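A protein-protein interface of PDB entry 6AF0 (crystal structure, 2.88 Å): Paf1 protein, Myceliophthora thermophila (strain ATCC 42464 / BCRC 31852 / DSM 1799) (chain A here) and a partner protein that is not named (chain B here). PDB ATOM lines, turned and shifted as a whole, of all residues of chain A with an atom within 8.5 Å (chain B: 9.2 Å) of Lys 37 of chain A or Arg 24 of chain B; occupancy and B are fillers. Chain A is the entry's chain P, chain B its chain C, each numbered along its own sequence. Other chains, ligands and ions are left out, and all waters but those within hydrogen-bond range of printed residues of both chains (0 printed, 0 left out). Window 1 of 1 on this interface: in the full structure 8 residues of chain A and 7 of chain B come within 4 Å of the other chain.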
ATOM      1  N   ILE A  34     -17.173  11.033   4.823  1.00  0.00           N
ATOM      2  CA  ILE A  34     -16.172   9.972   5.028  1.00  0.00           C
ATOM      3  C   ILE A  34     -16.872   8.630   5.179  1.00  0.00           C
ATOM      4  O   ILE A  34     -16.887   8.055   6.260  1.00  0.00           O
ATOM      5  CB  ILE A  34     -15.280  10.199   6.273  1.00  0.00           C
ATOM      6  CG1 ILE A  34     -14.686  11.615   6.290  1.00  0.00           C
ATOM      7  CG2 ILE A  34     -14.144   9.187   6.286  1.00  0.00           C
ATOM      8  CD1 ILE A  34     -13.679  11.865   7.406  1.00  0.00           C
ATOM      9  N   PRO A  35     -17.491   8.138   4.103  1.00  0.00           N
ATOM     10  CA  PRO A  35     -18.205   6.872   4.190  1.00  0.00           C
ATOM     11  C   PRO A  35     -17.289   5.669   4.505  1.00  0.00           C
ATOM     12  O   PRO A  35     -16.072   5.817   4.655  1.00  0.00           O
ATOM     13  CB  PRO A  35     -18.831   6.732   2.794  1.00  0.00           C
ATOM     14  CG  PRO A  35     -18.011   7.576   1.890  1.00  0.00           C
ATOM     15  CD  PRO A  35     -17.501   8.698   2.741  1.00  0.00           C
ATOM     16  N   PRO A  36     -17.869   4.474   4.612  1.00  0.00           N
ATOM     17  CA  PRO A  36     -17.064   3.264   4.666  1.00  0.00           C
ATOM     18  C   PRO A  36     -16.221   3.089   3.429  1.00  0.00           C
ATOM     19  O   PRO A  36     -16.498   3.695   2.405  1.00  0.00           O
ATOM     20  CB  PRO A  36     -18.110   2.156   4.737  1.00  0.00           C
ATOM     21  CG  PRO A  36     -19.245   2.785   5.432  1.00  0.00           C
ATOM     22  CD  PRO A  36     -19.268   4.219   4.973  1.00  0.00           C
ATOM     23  N   LYS A  37     -15.218   2.236   3.526  1.00  0.00           N
ATOM     24  CA  LYS A  37     -14.209   2.089   2.489  1.00  0.00           C
ATOM     25  C   LYS A  37     -14.279   0.722   1.879  1.00  0.00           C
ATOM     26  O   LYS A  37     -14.332  -0.259   2.590  1.00  0.00           O
ATOM     27  CB  LYS A  37     -12.823   2.308   3.094  1.00  0.00           C
ATOM     28  CG  LYS A  37     -12.620   3.687   3.715  1.00  0.00           C
ATOM     29  CD  LYS A  37     -11.583   3.688   4.820  1.00  0.00           C
ATOM     30  CE  LYS A  37     -11.465   5.048   5.476  1.00  0.00           C
ATOM     31  NZ  LYS A  37     -11.364   6.146   4.465  1.00  0.00           N
ATOM     32  N   LEU A  38     -14.293   0.668   0.554  1.00  0.00           N
ATOM     33  CA  LEU A  38     -14.303  -0.596  -0.179  1.00  0.00           C
ATOM     34  C   LEU A  38     -12.948  -1.207  -0.012  1.00  0.00           C
ATOM     35  O   LEU A  38     -11.958  -0.508   0.058  1.00  0.00           O
ATOM     36  CB  LEU A  38     -14.579  -0.417  -1.691  1.00  0.00           C
ATOM     37  CG  LEU A  38     -16.004  -0.422  -2.281  1.00  0.00           C
ATOM     38  CD1 LEU A  38     -16.817  -1.593  -1.746  1.00  0.00           C
ATOM     39  CD2 LEU A  38     -16.725   0.867  -1.968  1.00  0.00           C
ATOM     40  N   LEU A  39     -12.926  -2.528   0.071  1.00  0.00           N
ATOM     41  CA  LEU A  39     -11.684  -3.295   0.115  1.00  0.00           C
ATOM     42  C   LEU A  39     -11.510  -4.117  -1.153  1.00  0.00           C
ATOM     43  O   LEU A  39     -12.483  -4.455  -1.834  1.00  0.00           O
ATOM     44  CB  LEU A  39     -11.626  -4.171   1.371  1.00  0.00           C
ATOM     45  CG  LEU A  39     -10.586  -3.728   2.410  1.00  0.00           C
ATOM     46  CD1 LEU A  39     -10.353  -2.217   2.441  1.00  0.00           C
ATOM     47  CD2 LEU A  39     -10.994  -4.228   3.795  1.00  0.00           C
ATOM     48  N   ASP A  40     -10.256  -4.395  -1.490  1.00  0.00           N
ATOM     49  CA  ASP A  40      -9.958  -5.087  -2.735  1.00  0.00           C
ATOM     50  C   ASP A  40     -10.198  -6.577  -2.538  1.00  0.00           C
ATOM     51  O   ASP A  40      -9.592  -7.189  -1.671  1.00  0.00           O
ATOM     52  CB  ASP A  40      -8.518  -4.807  -3.196  1.00  0.00           C
ATOM     53  CG  ASP A  40      -8.430  -4.535  -4.682  1.00  0.00           C
ATOM     54  OD1 ASP A  40      -9.314  -5.007  -5.434  1.00  0.00           O
ATOM     55  OD2 ASP A  40      -7.482  -3.832  -5.093  1.00  0.00           O
ATOM     56  N   ILE A  41     -11.095  -7.151  -3.332  1.00  0.00           N
ATOM     57  CA  ILE A  41     -11.403  -8.587  -3.251  1.00  0.00           C
ATOM     58  C   ILE A  41     -10.509  -9.434  -4.167  1.00  0.00           C
ATOM     59  O   ILE A  41     -10.617  -9.331  -5.380  1.00  0.00           O
ATOM     60  CB  ILE A  41     -12.843  -8.869  -3.651  1.00  0.00           C
ATOM     61  CG1 ILE A  41     -13.801  -8.110  -2.725  1.00  0.00           C
ATOM     62  CG2 ILE A  41     -13.097 -10.365  -3.610  1.00  0.00           C
ATOM     63  CD1 ILE A  41     -15.258  -8.161  -3.156  1.00  0.00           C
ATOM     64  N   ILE B  19      -1.566   0.188   4.282  1.00  0.00           N
ATOM     65  CA  ILE B  19      -2.921  -0.034   4.802  1.00  0.00           C
ATOM     66  C   ILE B  19      -3.959   0.687   3.923  1.00  0.00           C
ATOM     67  O   ILE B  19      -4.995   0.121   3.561  1.00  0.00           O
ATOM     68  CB  ILE B  19      -3.050   0.407   6.280  1.00  0.00           C
ATOM     69  CG1 ILE B  19      -2.357  -0.602   7.196  1.00  0.00           C
ATOM     70  CG2 ILE B  19      -4.505   0.495   6.701  1.00  0.00           C
ATOM     71  CD1 ILE B  19      -2.464  -0.304   8.681  1.00  0.00           C
ATOM     72  N   TYR B  20      -3.666   1.936   3.577  1.00  0.00           N
ATOM     73  CA  TYR B  20      -4.528   2.723   2.705  1.00  0.00           C
ATOM     74  C   TYR B  20      -4.562   2.162   1.292  1.00  0.00           C
ATOM     75  O   TYR B  20      -5.538   2.349   0.565  1.00  0.00           O
ATOM     76  CB  TYR B  20      -4.045   4.174   2.645  1.00  0.00           C
ATOM     77  CG  TYR B  20      -4.137   4.972   3.940  1.00  0.00           C
ATOM     78  CD1 TYR B  20      -3.626   6.265   4.013  1.00  0.00           C
ATOM     79  CD2 TYR B  20      -4.721   4.441   5.088  1.00  0.00           C
ATOM     80  CE1 TYR B  20      -3.711   7.007   5.176  1.00  0.00           C
ATOM     81  CE2 TYR B  20      -4.801   5.178   6.256  1.00  0.00           C
ATOM     82  CZ  TYR B  20      -4.296   6.461   6.302  1.00  0.00           C
ATOM     83  OH  TYR B  20      -4.377   7.186   7.488  1.00  0.00           O
ATOM     84  N   SER B  21      -3.490   1.491   0.891  1.00  0.00           N
ATOM     85  CA  SER B  21      -3.400   0.922  -0.448  1.00  0.00           C
ATOM     86  C   SER B  21      -4.579  -0.006  -0.724  1.00  0.00           C
ATOM     87  O   SER B  21      -5.164   0.022  -1.811  1.00  0.00           O
ATOM     88  CB  SER B  21      -2.088   0.155  -0.608  1.00  0.00           C
ATOM     89  OG  SER B  21      -2.104  -1.017   0.183  1.00  0.00           O
ATOM     90  N   GLY B  22      -4.921  -0.813   0.278  1.00  0.00           N
ATOM     91  CA  GLY B  22      -6.026  -1.773   0.169  1.00  0.00           C
ATOM     92  C   GLY B  22      -7.418  -1.151   0.135  1.00  0.00           C
ATOM     93  O   GLY B  22      -8.387  -1.804  -0.273  1.00  0.00           O
ATOM     94  N   GLU B  23      -7.507   0.106   0.583  1.00  0.00           N
ATOM     95  CA  GLU B  23      -8.764   0.858   0.650  1.00  0.00           C
ATOM     96  C   GLU B  23      -9.097   1.495  -0.678  1.00  0.00           C
ATOM     97  O   GLU B  23      -8.203   1.981  -1.364  1.00  0.00           O
ATOM     98  CB  GLU B  23      -8.680   1.947   1.728  1.00  0.00           C
ATOM     99  CG  GLU B  23      -8.489   1.403   3.145  1.00  0.00           C
ATOM    100  CD  GLU B  23      -8.429   2.487   4.216  1.00  0.00           C
ATOM    101  OE1 GLU B  23      -8.335   3.683   3.864  1.00  0.00           O
ATOM    102  OE2 GLU B  23      -8.478   2.150   5.418  1.00  0.00           O
ATOM    103  N   ARG B  24     -10.387   1.488  -1.021  1.00  0.00           N
ATOM    104  CA  ARG B  24     -10.925   2.195  -2.196  1.00  0.00           C
ATOM    105  C   ARG B  24     -12.103   3.091  -1.773  1.00  0.00           C
ATOM    106  O   ARG B  24     -13.099   2.636  -1.228  1.00  0.00           O
ATOM    107  CB  ARG B  24     -11.332   1.202  -3.306  1.00  0.00           C
ATOM    108  CG  ARG B  24     -10.160   0.318  -3.744  1.00  0.00           C
ATOM    109  CD  ARG B  24     -10.348  -0.399  -5.079  1.00  0.00           C
ATOM    110  NE  ARG B  24     -11.498  -1.295  -5.079  1.00  0.00           N
ATOM    111  CZ  ARG B  24     -12.713  -0.967  -5.521  1.00  0.00           C
ATOM    112  NH1 ARG B  24     -12.958   0.239  -6.014  1.00  0.00           N
ATOM    113  NH2 ARG B  24     -13.701  -1.856  -5.466  1.00  0.00           N
ATOM    114  N   ARG B  25     -11.993   4.384  -2.011  1.00  0.00           N
ATOM    115  CA  ARG B  25     -13.017   5.287  -1.496  1.00  0.00           C
ATOM    116  C   ARG B  25     -14.320   5.098  -2.277  1.00  0.00           C
ATOM    117  O   ARG B  25     -14.306   4.686  -3.426  1.00  0.00           O
ATOM    118  CB  ARG B  25     -12.518   6.739  -1.534  1.00  0.00           C
ATOM    119  CG  ARG B  25     -12.667   7.480  -0.211  1.00  0.00           C
ATOM    120  CD  ARG B  25     -11.542   8.484   0.015  1.00  0.00           C
ATOM    121  NE  ARG B  25     -10.365   7.893   0.666  1.00  0.00           N
ATOM    122  CZ  ARG B  25      -9.100   8.251   0.429  1.00  0.00           C
ATOM    123  NH1 ARG B  25      -8.806   9.187  -0.469  1.00  0.00           N
ATOM    124  NH2 ARG B  25      -8.107   7.656   1.080  1.00  0.00           N
ATOM    125  N   MET B  26     -15.452   5.349  -1.639  1.00  0.00           N
ATOM    126  CA  MET B  26     -16.718   5.366  -2.375  1.00  0.00           C
ATOM    127  C   MET B  26     -17.469   6.655  -2.174  1.00  0.00           C
ATOM    128  O   MET B  26     -18.656   6.739  -2.489  1.00  0.00           O
ATOM    129  CB  MET B  26     -17.606   4.212  -1.972  1.00  0.00           C
ATOM    130  CG  MET B  26     -17.960   4.175  -0.501  1.00  0.00           C
ATOM    131  SD  MET B  26     -18.721   2.594  -0.080  1.00  0.00           S
ATOM    132  CE  MET B  26     -20.001   2.473  -1.329  1.00  0.00           C
ATOM    133  N   GLY B  27     -16.766   7.660  -1.661  1.00  0.00           N
ATOM    134  CA  GLY B  27     -17.298   9.013  -1.526  1.00  0.00           C
ATOM    135  C   GLY B  27     -16.305   9.859  -0.761  1.00  0.00           C
ATOM    136  O   GLY B  27     -15.521   9.358   0.070  1.00  0.00           O
ATOM    137  N   ASP B  28     -16.338  11.151  -1.025  1.00  0.00           N
ATOM    138  CA  ASP B  28     -15.389  12.063  -0.421  1.00  0.00           C
ATOM    139  C   ASP B  28     -16.047  13.427  -0.295  1.00  0.00           C
ATOM    140  O   ASP B  28     -17.250  13.548  -0.478  1.00  0.00           O
ATOM    141  CB  ASP B  28     -14.127  12.111  -1.292  1.00  0.00           C
ATOM    142  CG  ASP B  28     -14.419  12.459  -2.733  1.00  0.00           C
ATOM    143  OD1 ASP B  28     -15.425  13.169  -3.015  1.00  0.00           O
ATOM    144  OD2 ASP B  28     -13.609  12.032  -3.581  1.00  0.00           O
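The side-chain amino group (NZ) of Lys 37 of chain A is in salt-bridge range of the side-chain carboxylate (OE1) of Glu 23 of chain B (3.9 Å). N of Arg 24 of chain B is in hydrogen-bond range of O of Leu 38 of chain A, 2.8 Å away. N of Asp 40 of chain A is in hydrogen-bond range of O of Gly 22 of chain B (3.4 Å). The backbone carbonyl oxygen of Pro 36 of chain A lies close to the side-chain sulfur of Met 26 of chain B (3.5 Å).
Among the printed residues, merely in contact across the chains: Leu 38 of chain A with Met 26 of chain B, Leu 39 of chain A with Gly 22 of chain B, Pro 35 of chain A with Gly 27 of chain B, Leu 38 of chain A with Glu 23 of chain B, Leu 38 of chain A with Gly 22 of chain B, Lys 37 of chain A with Arg 24 of chain B and Leu 39 of chain A with Glu 23 of chain B.
Of the printed residues of chain B, Pro 35 of chain A touches Gly 27. Of chain B, only Met 26 comes within 4 Å of Pro 36 of chain A. Of chain B, only Glu 23 (3.4 Å) and Arg 24 (3.8 Å) come within 4 Å of Lys 37 of chain A. Printed residues of chain B within 4 Å of Leu 38 of chain A: Gly 22 (3.8 Å), Glu 23 (3.5 Å), Arg 24 (2.8 Å) and Met 26 (3.2 Å). Of the printed residues of chain B, Leu 39 of chain A touches Gly 22 and Glu 23. Of the printed residues of chain B, Asp 40 of chain A touches Gly 22. Glu 23 of chain B touches just these residues of chain A: Lys 37 (3.4 Å), Leu 38 (3.5 Å) and Leu 39 (3.9 Å). Of chain A, only Lys 37 (3.8 Å) and Leu 38 (2.8 Å) come within 4 Å of Arg 24 of chain B. Printed residues of chain A within 4 Å of Met 26 of chain B: Pro 36 (3.3 Å) and Leu 38 (3.2 Å). Printed residues of chain A within 4 Å of Gly 27 of chain B: Pro 35 (3.4 Å). The nearest residue of chain B that does not touch Lys 37 of chain A is Arg 25 of chain B (4.3 Å). The nearest residue of chain A that does not touch Arg 24 of chain B is Asp 40 of chain A (4.3 Å).
Of the 10 printed residues of chain B, 5 touch a printed residue of chain A. Printed residues of chain A that touch a printed residue of chain B: Pro 35, Pro 36, Lys 37, Leu 38, Leu 39 and Asp 40. Among the printed residues, Asp or Glu carboxylates within 4 Å of a Lys or Arg side-chain nitrogen of the other chain: Lys 37 of chain A with Glu 23 of chain B (3.9 Å).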
